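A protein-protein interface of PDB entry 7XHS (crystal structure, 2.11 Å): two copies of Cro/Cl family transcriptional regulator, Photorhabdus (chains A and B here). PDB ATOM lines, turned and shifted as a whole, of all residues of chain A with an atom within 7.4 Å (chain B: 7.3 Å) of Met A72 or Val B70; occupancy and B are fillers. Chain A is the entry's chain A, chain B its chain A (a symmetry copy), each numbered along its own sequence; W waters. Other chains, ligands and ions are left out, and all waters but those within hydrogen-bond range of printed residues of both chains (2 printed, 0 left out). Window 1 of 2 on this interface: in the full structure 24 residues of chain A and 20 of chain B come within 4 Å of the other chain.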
ATOM      1  N   ILE A  26      28.963  -2.113   7.557  1.00  0.00           N
ATOM      2  CA  ILE A  26      28.654  -2.714   8.855  1.00  0.00           C
ATOM      3  C   ILE A  26      27.607  -3.801   8.628  1.00  0.00           C
ATOM      4  O   ILE A  26      26.405  -3.514   8.543  1.00  0.00           O
ATOM      5  CB  ILE A  26      28.151  -1.674   9.860  1.00  0.00           C
ATOM      6  CG1 ILE A  26      29.113  -0.480   9.953  1.00  0.00           C
ATOM      7  CG2 ILE A  26      27.974  -2.316  11.216  1.00  0.00           C
ATOM      8  CD1 ILE A  26      30.530  -0.828  10.412  1.00  0.00           C
ATOM      9  N   MET A  29      25.599  -6.679  13.821  1.00  0.00           N
ATOM     10  CA  MET A  29      25.900  -6.204  15.175  1.00  0.00           C
ATOM     11  C   MET A  29      25.218  -7.138  16.158  1.00  0.00           C
ATOM     12  O   MET A  29      24.031  -7.441  16.004  1.00  0.00           O
ATOM     13  CB  MET A  29      25.421  -4.753  15.405  1.00  0.00           C
ATOM     14  CG  MET A  29      26.126  -3.712  14.518  1.00  0.00           C
ATOM     15  SD  MET A  29      25.787  -1.971  14.868  1.00  0.00           S
ATOM     16  CE  MET A  29      25.936  -1.858  16.656  1.00  0.00           C
ATOM     17  N   VAL A  31      24.316  -7.428  20.047  1.00  0.00           N
ATOM     18  CA  VAL A  31      24.217  -6.663  21.285  1.00  0.00           C
ATOM     19  C   VAL A  31      23.979  -7.654  22.415  1.00  0.00           C
ATOM     20  O   VAL A  31      22.954  -8.345  22.442  1.00  0.00           O
ATOM     21  CB  VAL A  31      23.086  -5.623  21.196  1.00  0.00           C
ATOM     22  CG1 VAL A  31      23.052  -4.709  22.421  1.00  0.00           C
ATOM     23  CG2 VAL A  31      23.228  -4.815  19.916  1.00  0.00           C
ATOM     24  N   VAL A  39      29.041  -5.703  22.901  1.00  0.00           N
ATOM     25  CA  VAL A  39      28.517  -5.621  21.538  1.00  0.00           C
ATOM     26  C   VAL A  39      29.662  -5.873  20.560  1.00  0.00           C
ATOM     27  O   VAL A  39      30.719  -5.242  20.642  1.00  0.00           O
ATOM     28  CB  VAL A  39      27.791  -4.282  21.282  1.00  0.00           C
ATOM     29  CG1 VAL A  39      28.703  -3.088  21.561  1.00  0.00           C
ATOM     30  CG2 VAL A  39      27.285  -4.225  19.827  1.00  0.00           C
ATOM     31  N   VAL A  41      30.802  -6.038  16.539  1.00  0.00           N
ATOM     32  CA  VAL A  41      30.481  -5.475  15.223  1.00  0.00           C
ATOM     33  C   VAL A  41      31.210  -6.275  14.143  1.00  0.00           C
ATOM     34  O   VAL A  41      32.447  -6.361  14.155  1.00  0.00           O
ATOM     35  CB  VAL A  41      30.893  -3.995  15.148  1.00  0.00           C
ATOM     36  CG1 VAL A  41      30.380  -3.342  13.882  1.00  0.00           C
ATOM     37  CG2 VAL A  41      30.450  -3.258  16.397  1.00  0.00           C
ATOM     38  N   ALA A  66      27.231   6.690  21.637  1.00  0.00           N
ATOM     39  CA  ALA A  66      27.240   7.491  20.415  1.00  0.00           C
ATOM     40  C   ALA A  66      27.850   6.716  19.249  1.00  0.00           C
ATOM     41  O   ALA A  66      27.317   6.746  18.133  1.00  0.00           O
ATOM     42  CB  ALA A  66      27.991   8.806  20.642  1.00  0.00           C
ATOM     43  N   ILE A  67      28.964   6.011  19.488  1.00  0.00           N
ATOM     44  CA  ILE A  67      29.549   5.162  18.452  1.00  0.00           C
ATOM     45  C   ILE A  67      28.613   4.013  18.097  1.00  0.00           C
ATOM     46  O   ILE A  67      28.473   3.644  16.921  1.00  0.00           O
ATOM     47  CB  ILE A  67      30.931   4.657  18.909  1.00  0.00           C
ATOM     48  CG1 ILE A  67      31.875   5.839  19.129  1.00  0.00           C
ATOM     49  CG2 ILE A  67      31.520   3.653  17.914  1.00  0.00           C
ATOM     50  CD1 ILE A  67      32.506   6.395  17.861  1.00  0.00           C
ATOM     51  N   TYR A  68      27.950   3.432  19.106  1.00  0.00           N
ATOM     52  CA  TYR A  68      26.987   2.363  18.851  1.00  0.00           C
ATOM     53  C   TYR A  68      25.859   2.824  17.927  1.00  0.00           C
ATOM     54  O   TYR A  68      25.389   2.059  17.079  1.00  0.00           O
ATOM     55  CB  TYR A  68      26.420   1.868  20.178  1.00  0.00           C
ATOM     56  CG  TYR A  68      25.219   0.939  20.116  1.00  0.00           C
ATOM     57  CD1 TYR A  68      23.952   1.377  20.498  1.00  0.00           C
ATOM     58  CD2 TYR A  68      25.362  -0.394  19.770  1.00  0.00           C
ATOM     59  CE1 TYR A  68      22.853   0.519  20.479  1.00  0.00           C
ATOM     60  CE2 TYR A  68      24.261  -1.272  19.755  1.00  0.00           C
ATOM     61  CZ  TYR A  68      23.016  -0.809  20.105  1.00  0.00           C
ATOM     62  OH  TYR A  68      21.942  -1.680  20.108  1.00  0.00           O
ATOM     63  N   LYS A  69      25.412   4.071  18.068  1.00  0.00           N
ATOM     64  CA  LYS A  69      24.259   4.514  17.283  1.00  0.00           C
ATOM     65  C   LYS A  69      24.607   4.762  15.824  1.00  0.00           C
ATOM     66  O   LYS A  69      23.832   4.380  14.934  1.00  0.00           O
ATOM     67  CB  LYS A  69      23.670   5.758  17.901  1.00  0.00           C
ATOM     68  CG  LYS A  69      23.243   5.421  19.253  1.00  0.00           C
ATOM     69  CD  LYS A  69      22.501   6.477  19.930  1.00  0.00           C
ATOM     70  CE  LYS A  69      22.722   6.177  21.380  1.00  0.00           C
ATOM     71  NZ  LYS A  69      21.843   6.908  22.257  1.00  0.00           N
ATOM     72  N   VAL A  70      25.744   5.413  15.546  1.00  0.00           N
ATOM     73  CA  VAL A  70      26.084   5.663  14.146  1.00  0.00           C
ATOM     74  C   VAL A  70      26.348   4.345  13.413  1.00  0.00           C
ATOM     75  O   VAL A  70      25.951   4.179  12.255  1.00  0.00           O
ATOM     76  CB  VAL A  70      27.263   6.646  14.021  1.00  0.00           C
ATOM     77  CG1 VAL A  70      28.534   6.127  14.731  1.00  0.00           C
ATOM     78  CG2 VAL A  70      27.519   6.954  12.539  1.00  0.00           C
ATOM     79  N   LEU A  71      26.976   3.375  14.080  1.00  0.00           N
ATOM     80  CA  LEU A  71      27.186   2.071  13.446  1.00  0.00           C
ATOM     81  C   LEU A  71      25.856   1.412  13.098  1.00  0.00           C
ATOM     82  O   LEU A  71      25.668   0.897  11.984  1.00  0.00           O
ATOM     83  CB  LEU A  71      27.998   1.166  14.367  1.00  0.00           C
ATOM     84  CG  LEU A  71      29.460   1.545  14.531  1.00  0.00           C
ATOM     85  CD1 LEU A  71      30.053   0.750  15.683  1.00  0.00           C
ATOM     86  CD2 LEU A  71      30.233   1.309  13.226  1.00  0.00           C
ATOM     87  N   MET A  72      24.917   1.434  14.042  1.00  0.00           N
ATOM     88  CA  MET A  72      23.603   0.824  13.841  1.00  0.00           C
ATOM     89  C   MET A  72      22.857   1.470  12.686  1.00  0.00           C
ATOM     90  O   MET A  72      22.242   0.779  11.866  1.00  0.00           O
ATOM     91  CB  MET A  72      22.790   0.974  15.114  1.00  0.00           C
ATOM     92  CG  MET A  72      21.382   0.480  15.063  1.00  0.00           C
ATOM     93  SD  MET A  72      21.356  -1.294  14.993  1.00  0.00           S
ATOM     94  CE  MET A  72      21.609  -1.526  16.744  1.00  0.00           C
ATOM     95  N   GLU A  73      22.857   2.808  12.644  1.00  0.00           N
ATOM     96  CA  GLU A  73      22.215   3.528  11.550  1.00  0.00           C
ATOM     97  C   GLU A  73      22.861   3.176  10.216  1.00  0.00           C
ATOM     98  O   GLU A  73      22.171   3.032   9.202  1.00  0.00           O
ATOM     99  CB  GLU A  73      22.288   5.039  11.798  1.00  0.00           C
ATOM    100  CG  GLU A  73      21.564   5.550  13.062  1.00  0.00           C
ATOM    101  CD  GLU A  73      20.093   5.854  12.846  1.00  0.00           C
ATOM    102  OE1 GLU A  73      19.777   6.918  12.260  1.00  0.00           O
ATOM    103  OE2 GLU A  73      19.247   5.047  13.286  1.00  0.00           O
ATOM    104  N   ALA A  74      24.187   3.021  10.204  1.00  0.00           N
ATOM    105  CA  ALA A  74      24.886   2.652   8.977  1.00  0.00           C
ATOM    106  C   ALA A  74      24.470   1.265   8.496  1.00  0.00           C
ATOM    107  O   ALA A  74      24.350   1.030   7.289  1.00  0.00           O
ATOM    108  CB  ALA A  74      26.391   2.701   9.215  1.00  0.00           C
ATOM    109  N   LEU A  75      24.271   0.327   9.428  1.00  0.00           N
ATOM    110  CA  LEU A  75      23.801  -1.003   9.050  1.00  0.00           C
ATOM    111  C   LEU A  75      22.378  -0.939   8.496  1.00  0.00           C
ATOM    112  O   LEU A  75      22.078  -1.506   7.435  1.00  0.00           O
ATOM    113  CB  LEU A  75      23.883  -1.946  10.259  1.00  0.00           C
ATOM    114  CG  LEU A  75      23.377  -3.397  10.124  1.00  0.00           C
ATOM    115  CD1 LEU A  75      24.061  -4.305  11.144  1.00  0.00           C
ATOM    116  CD2 LEU A  75      21.869  -3.510  10.273  1.00  0.00           C
ATOM    117  N   CYS A  76      21.483  -0.253   9.203  1.00  0.00           N
ATOM    118  CA  CYS A  76      20.083  -0.224   8.799  1.00  0.00           C
ATOM    119  C   CYS A  76      19.846   0.601   7.537  1.00  0.00           C
ATOM    120  O   CYS A  76      18.866   0.352   6.832  1.00  0.00           O
ATOM    121  CB  CYS A  76      19.203   0.320   9.932  1.00  0.00           C
ATOM    122  SG  CYS A  76      19.100  -0.706  11.412  1.00  0.00           S
ATOM    123  N   ALA A  77      20.704   1.571   7.230  1.00  0.00           N
ATOM    124  CA  ALA A  77      20.546   2.329   5.994  1.00  0.00           C
ATOM    125  C   ALA A  77      21.314   1.718   4.836  1.00  0.00           C
ATOM    126  O   ALA A  77      21.206   2.211   3.706  1.00  0.00           O
ATOM    127  CB  ALA A  77      20.986   3.785   6.195  1.00  0.00           C
ATOM    128  N   LYS A  78      22.070   0.649   5.090  1.00  0.00           N
ATOM    129  CA  LYS A  78      22.895  -0.002   4.078  1.00  0.00           C
ATOM    130  C   LYS A  78      23.874   0.990   3.457  1.00  0.00           C
ATOM    131  O   LYS A  78      23.941   1.153   2.241  1.00  0.00           O
ATOM    132  CB  LYS A  78      22.029  -0.667   3.010  1.00  0.00           C
ATOM    133  CG  LYS A  78      21.102  -1.763   3.544  1.00  0.00           C
ATOM    134  CD  LYS A  78      20.090  -2.150   2.462  1.00  0.00           C
ATOM    135  CE  LYS A  78      19.634  -3.590   2.583  1.00  0.00           C
ATOM    136  NZ  LYS A  78      19.106  -3.874   3.936  1.00  0.00           N
ATOM    137  N   ILE B  26       9.872  -8.096  15.139  1.00  0.00           N
ATOM    138  CA  ILE B  26       9.417  -7.225  16.224  1.00  0.00           C
ATOM    139  C   ILE B  26       8.209  -6.442  15.718  1.00  0.00           C
ATOM    140  O   ILE B  26       8.359  -5.416  15.039  1.00  0.00           O
ATOM    141  CB  ILE B  26      10.523  -6.278  16.697  1.00  0.00           C
ATOM    142  CG1 ILE B  26      11.810  -7.047  17.030  1.00  0.00           C
ATOM    143  CG2 ILE B  26      10.049  -5.497  17.900  1.00  0.00           C
ATOM    144  CD1 ILE B  26      11.670  -8.086  18.143  1.00  0.00           C
ATOM    145  N   MET B  29       5.845  -2.293  19.778  1.00  0.00           N
ATOM    146  CA  MET B  29       6.520  -1.903  21.019  1.00  0.00           C
ATOM    147  C   MET B  29       5.658  -0.863  21.711  1.00  0.00           C
ATOM    148  O   MET B  29       5.219   0.100  21.075  1.00  0.00           O
ATOM    149  CB  MET B  29       7.933  -1.332  20.761  1.00  0.00           C
ATOM    150  CG  MET B  29       8.915  -2.345  20.146  1.00  0.00           C
ATOM    151  SD  MET B  29      10.643  -1.832  20.010  1.00  0.00           S
ATOM    152  CE  MET B  29      11.003  -1.112  21.618  1.00  0.00           C
ATOM    153  N   GLY B  64      19.648  -1.297  29.085  1.00  0.00           N
ATOM    154  CA  GLY B  64      18.271  -1.334  28.621  1.00  0.00           C
ATOM    155  C   GLY B  64      18.038  -0.425  27.433  1.00  0.00           C
ATOM    156  O   GLY B  64      17.347  -0.800  26.481  1.00  0.00           O
ATOM    157  N   MET B  65      18.627   0.778  27.459  1.00  0.00           N
ATOM    158  CA  MET B  65      18.518   1.692  26.321  1.00  0.00           C
ATOM    159  C   MET B  65      19.092   1.068  25.051  1.00  0.00           C
ATOM    160  O   MET B  65      18.542   1.250  23.965  1.00  0.00           O
ATOM    161  CB  MET B  65      19.236   3.014  26.618  1.00  0.00           C
ATOM    162  CG  MET B  65      18.506   4.062  27.490  1.00  0.00           C
ATOM    163  SD  MET B  65      16.850   4.564  26.950  1.00  0.00           S
ATOM    164  CE  MET B  65      17.262   5.595  25.584  1.00  0.00           C
ATOM    165  N   ALA B  66      20.215   0.346  25.164  1.00  0.00           N
ATOM    166  CA  ALA B  66      20.846  -0.218  23.973  1.00  0.00           C
ATOM    167  C   ALA B  66      19.992  -1.330  23.367  1.00  0.00           C
ATOM    168  O   ALA B  66      19.822  -1.389  22.143  1.00  0.00           O
ATOM    169  CB  ALA B  66      22.249  -0.736  24.305  1.00  0.00           C
ATOM    170  N   ILE B  67      19.440  -2.216  24.206  1.00  0.00           N
ATOM    171  CA  ILE B  67      18.528  -3.246  23.714  1.00  0.00           C
ATOM    172  C   ILE B  67      17.253  -2.622  23.158  1.00  0.00           C
ATOM    173  O   ILE B  67      16.722  -3.067  22.129  1.00  0.00           O
ATOM    174  CB  ILE B  67      18.229  -4.259  24.836  1.00  0.00           C
ATOM    175  CG1 ILE B  67      19.519  -4.953  25.273  1.00  0.00           C
ATOM    176  CG2 ILE B  67      17.169  -5.278  24.405  1.00  0.00           C
ATOM    177  CD1 ILE B  67      19.967  -6.094  24.370  1.00  0.00           C
ATOM    178  N   TYR B  68      16.744  -1.577  23.824  1.00  0.00           N
ATOM    179  CA  TYR B  68      15.559  -0.880  23.329  1.00  0.00           C
ATOM    180  C   TYR B  68      15.779  -0.312  21.926  1.00  0.00           C
ATOM    181  O   TYR B  68      14.866  -0.321  21.094  1.00  0.00           O
ATOM    182  CB  TYR B  68      15.186   0.234  24.303  1.00  0.00           C
ATOM    183  CG  TYR B  68      14.141   1.236  23.843  1.00  0.00           C
ATOM    184  CD1 TYR B  68      14.494   2.544  23.517  1.00  0.00           C
ATOM    185  CD2 TYR B  68      12.795   0.910  23.825  1.00  0.00           C
ATOM    186  CE1 TYR B  68      13.534   3.479  23.130  1.00  0.00           C
ATOM    187  CE2 TYR B  68      11.816   1.847  23.444  1.00  0.00           C
ATOM    188  CZ  TYR B  68      12.191   3.121  23.097  1.00  0.00           C
ATOM    189  OH  TYR B  68      11.224   4.043  22.742  1.00  0.00           O
ATOM    190  N   LYS B  69      16.982   0.183  21.639  1.00  0.00           N
ATOM    191  CA  LYS B  69      17.200   0.838  20.348  1.00  0.00           C
ATOM    192  C   LYS B  69      17.289  -0.153  19.199  1.00  0.00           C
ATOM    193  O   LYS B  69      16.718   0.097  18.126  1.00  0.00           O
ATOM    194  CB  LYS B  69      18.447   1.684  20.411  1.00  0.00           C
ATOM    195  CG  LYS B  69      18.248   2.691  21.445  1.00  0.00           C
ATOM    196  CD  LYS B  69      19.303   3.695  21.518  1.00  0.00           C
ATOM    197  CE  LYS B  69      19.218   4.179  22.932  1.00  0.00           C
ATOM    198  NZ  LYS B  69      19.965   5.388  23.169  1.00  0.00           N
ATOM    199  N   VAL B  70      18.010  -1.268  19.378  1.00  0.00           N
ATOM    200  CA  VAL B  70      18.108  -2.223  18.275  1.00  0.00           C
ATOM    201  C   VAL B  70      16.740  -2.840  17.975  1.00  0.00           C
ATOM    202  O   VAL B  70      16.385  -3.044  16.809  1.00  0.00           O
ATOM    203  CB  VAL B  70      19.181  -3.293  18.554  1.00  0.00           C
ATOM    204  CG1 VAL B  70      18.891  -4.089  19.846  1.00  0.00           C
ATOM    205  CG2 VAL B  70      19.318  -4.212  17.332  1.00  0.00           C
ATOM    206  N   LEU B  71      15.933  -3.104  19.004  1.00  0.00           N
ATOM    207  CA  LEU B  71      14.586  -3.625  18.762  1.00  0.00           C
ATOM    208  C   LEU B  71      13.756  -2.637  17.949  1.00  0.00           C
ATOM    209  O   LEU B  71      13.084  -3.014  16.976  1.00  0.00           O
ATOM    210  CB  LEU B  71      13.897  -3.928  20.088  1.00  0.00           C
ATOM    211  CG  LEU B  71      14.439  -5.127  20.847  1.00  0.00           C
ATOM    212  CD1 LEU B  71      13.866  -5.124  22.255  1.00  0.00           C
ATOM    213  CD2 LEU B  71      14.115  -6.431  20.108  1.00  0.00           C
ATOM    214  N   MET B  72      13.806  -1.363  18.333  1.00  0.00           N
ATOM    215  CA  MET B  72      13.045  -0.318  17.647  1.00  0.00           C
ATOM    216  C   MET B  72      13.456  -0.191  16.191  1.00  0.00           C
ATOM    217  O   MET B  72      12.605  -0.058  15.303  1.00  0.00           O
ATOM    218  CB  MET B  72      13.276   1.004  18.354  1.00  0.00           C
ATOM    219  CG  MET B  72      12.640   2.205  17.737  1.00  0.00           C
ATOM    220  SD  MET B  72      10.879   2.146  17.954  1.00  0.00           S
ATOM    221  CE  MET B  72      10.904   2.747  19.634  1.00  0.00           C
ATOM    222  N   GLU B  73      14.770  -0.174  15.935  1.00  0.00           N
ATOM    223  CA  GLU B  73      15.272  -0.108  14.568  1.00  0.00           C
ATOM    224  C   GLU B  73      14.816  -1.318  13.763  1.00  0.00           C
ATOM    225  O   GLU B  73      14.472  -1.195  12.584  1.00  0.00           O
ATOM    226  CB  GLU B  73      16.802  -0.013  14.572  1.00  0.00           C
ATOM    227  CG  GLU B  73      17.397   1.238  15.254  1.00  0.00           C
ATOM    228  CD  GLU B  73      17.520   2.439  14.334  1.00  0.00           C
ATOM    229  OE1 GLU B  73      18.461   2.469  13.504  1.00  0.00           O
ATOM    230  OE2 GLU B  73      16.696   3.369  14.456  1.00  0.00           O
ATOM    231  N   ALA B  74      14.797  -2.495  14.393  1.00  0.00           N
ATOM    232  CA  ALA B  74      14.344  -3.703  13.709  1.00  0.00           C
ATOM    233  C   ALA B  74      12.870  -3.603  13.323  1.00  0.00           C
ATOM    234  O   ALA B  74      12.469  -4.076  12.254  1.00  0.00           O
ATOM    235  CB  ALA B  74      14.576  -4.913  14.606  1.00  0.00           C
ATOM    236  N   LEU B  75      12.046  -3.011  14.195  1.00  0.00           N
ATOM    237  CA  LEU B  75      10.638  -2.814  13.865  1.00  0.00           C
ATOM    238  C   LEU B  75      10.485  -1.823  12.711  1.00  0.00           C
ATOM    239  O   LEU B  75       9.757  -2.078  11.741  1.00  0.00           O
ATOM    240  CB  LEU B  75       9.874  -2.340  15.109  1.00  0.00           C
ATOM    241  CG  LEU B  75       8.374  -1.999  14.993  1.00  0.00           C
ATOM    242  CD1 LEU B  75       7.680  -2.143  16.346  1.00  0.00           C
ATOM    243  CD2 LEU B  75       8.129  -0.604  14.442  1.00  0.00           C
ATOM    244  N   CYS B  76      11.163  -0.681  12.801  1.00  0.00           N
ATOM    245  CA  CYS B  76      10.997   0.361  11.795  1.00  0.00           C
ATOM    246  C   CYS B  76      11.622  -0.006  10.451  1.00  0.00           C
ATOM    247  O   CYS B  76      11.185   0.516   9.424  1.00  0.00           O
ATOM    248  CB  CYS B  76      11.591   1.687  12.284  1.00  0.00           C
ATOM    249  SG  CYS B  76      10.762   2.451  13.693  1.00  0.00           S
ATOM    250  N   VAL B  81      15.227 -10.452  13.002  1.00  0.00           N
ATOM    251  CA  VAL B  81      16.351 -10.439  13.934  1.00  0.00           C
ATOM    252  C   VAL B  81      16.365 -11.755  14.701  1.00  0.00           C
ATOM    253  O   VAL B  81      15.454 -12.578  14.589  1.00  0.00           O
ATOM    254  CB  VAL B  81      16.297  -9.259  14.932  1.00  0.00           C
ATOM    255  CG1 VAL B  81      16.409  -7.919  14.205  1.00  0.00           C
ATOM    256  CG2 VAL B  81      15.029  -9.327  15.795  1.00  0.00           C
ATOM    257  N   CYS B  99      19.524 -10.430  24.666  1.00  0.00           N
ATOM    258  CA  CYS B  99      20.472 -10.356  23.559  1.00  0.00           C
ATOM    259  C   CYS B  99      19.717 -10.190  22.240  1.00  0.00           C
ATOM    260  O   CYS B  99      18.700 -10.855  22.008  1.00  0.00           O
ATOM    261  CB  CYS B  99      21.348 -11.616  23.528  1.00  0.00           C
ATOM    262  SG  CYS B  99      22.484 -11.758  22.139  1.00  0.00           S
ATOM    263  N   VAL B 100      20.204  -9.295  21.379  1.00  0.00           N
ATOM    264  CA  VAL B 100      19.639  -9.122  20.042  1.00  0.00           C
ATOM    265  C   VAL B 100      20.771  -9.089  19.026  1.00  0.00           C
ATOM    266  O   VAL B 100      21.800  -8.438  19.245  1.00  0.00           O
ATOM    267  CB  VAL B 100      18.774  -7.844  19.922  1.00  0.00           C
ATOM    268  CG1 VAL B 100      18.174  -7.746  18.542  1.00  0.00           C
ATOM    269  CG2 VAL B 100      17.654  -7.838  20.969  1.00  0.00           C
ATOM    270  N   GLU B 101      20.584  -9.803  17.919  1.00  0.00           N
ATOM    271  CA  GLU B 101      21.511  -9.771  16.798  1.00  0.00           C
ATOM    272  C   GLU B 101      20.777  -9.305  15.550  1.00  0.00           C
ATOM    273  O   GLU B 101      19.680  -9.783  15.258  1.00  0.00           O
ATOM    274  CB  GLU B 101      22.150 -11.135  16.562  1.00  0.00           C
ATOM    275  CG  GLU B 101      23.361 -11.060  15.661  1.00  0.00           C
ATOM    276  CD  GLU B 101      23.690 -12.385  14.995  1.00  0.00           C
ATOM    277  OE1 GLU B 101      24.204 -13.296  15.689  1.00  0.00           O
ATOM    278  OE2 GLU B 101      23.431 -12.509  13.776  1.00  0.00           O
ATOM    279  N   ILE B 102      21.391  -8.383  14.820  1.00  0.00           N
ATOM    280  CA  ILE B 102      20.805  -7.756  13.641  1.00  0.00           C
ATOM    281  C   ILE B 102      21.853  -7.773  12.533  1.00  0.00           C
ATOM    282  O   ILE B 102      23.049  -7.616  12.801  1.00  0.00           O
ATOM    283  CB  ILE B 102      20.336  -6.321  13.982  1.00  0.00           C
ATOM    284  CG1 ILE B 102      19.372  -5.767  12.925  1.00  0.00           C
ATOM    285  CG2 ILE B 102      21.539  -5.382  14.259  1.00  0.00           C
ATOM    286  CD1 ILE B 102      18.853  -4.373  13.261  1.00  0.00           C
HETATM  287  O   HOH W   1      20.661   7.454  24.390  1.00  0.00           O
HETATM  288  O   HOH W   2      19.538   4.193  16.334  1.00  0.00           O
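The side-chain carboxylate of Glu A73 lies close to the side-chain carboxylate of Glu B73, at 2.7 Å. The side-chain hydroxyl (OH) of Tyr A68 lies within hydrogen-bond range of the backbone carbonyl oxygen (O) of Ala B66. The backbone carbonyl oxygen (O) of Ile B102 sits at hydrogen-bond distance from the backbone NH (N) of Met A29 (2.9 Å). The side-chain amino group of Lys A69 sits close to the side-chain amino group of Lys B69. The backbone carbonyl oxygen (O) of Val B100 lies within hydrogen-bond range of the backbone NH (N) of Val A31. O of Val A31 lies close to SG of Cys B99 (3.5 Å).
O of Met A72 sits at hydrogen-bond distance from SG of Cys A76, 3.5 Å away. N of Met A72 sits at hydrogen-bond distance from SD of Met A29.
Among the printed residues, merely in contact across the chains: Met A29 with Glu B101 (3.5 Å), Val A31 with Ile B67 (3.9 Å), Tyr A68 with Val B70 (3.6 Å), Met A72 with Val B70 (3.5 Å), Met A72 with Glu B73 (3.9 Å), Leu A75 with Ile B102 (3.8 Å) and Cys A76 with Glu B73 (3.9 Å).
Met A72 touches just these residues of chain B: Val B70 (3.5 Å) and Glu B73 (3.9 Å). Val B70 touches just these residues of chain A: Tyr A68 and Met A72. Printed residues of chain B within 4 Å of Leu A75: Ile B102. Of the printed residues of chain B, Glu A73 touches Glu B73. Printed residues of chain B within 4 Å of Cys A76: Glu B73. The nearest residue of chain A that does not touch Val B70 is Val A31 (4.4 Å).
Along chain B the printed residues that touch a printed residue of chain A span positions 66 to 102. Among the printed residues, 13 pairs touch across the chains. Among the printed residues, no Asp or Glu carboxylate lies within 4 Å of a Lys or Arg side-chain nitrogen of the other chain.
Tyr A68 touches Ala B66, but with the chains exchanged Ala A66 does not touch Tyr B68 (13.4 Å). Tyr A68 touches Val B70, but with the chains exchanged Val A70 does not touch Tyr B68 (13.1 Å). Met A72 touches Val B70, but with the chains exchanged Val A70 does not touch Met B72 (13.5 Å). Glu A73 touches its own counterpart, Glu B73. Positions printed for both chains: 26, 29, 66, 67, 68, 69, 70, 71, 72, 73, 74, 75 and 76. Of the 13 pairs that touch across the chains among the printed residues, 2 have their exchanged pair printed and touching as well.
Water W1 lies within hydrogen-bond range of NZ of Lys B69 (2.5 Å) and NZ of Lys A69 (2.5 Å). Water W2 lies within hydrogen-bond range of OE2 of Glu A73 (3.2 Å) and OE1 of Glu B73 (3.5 Å).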
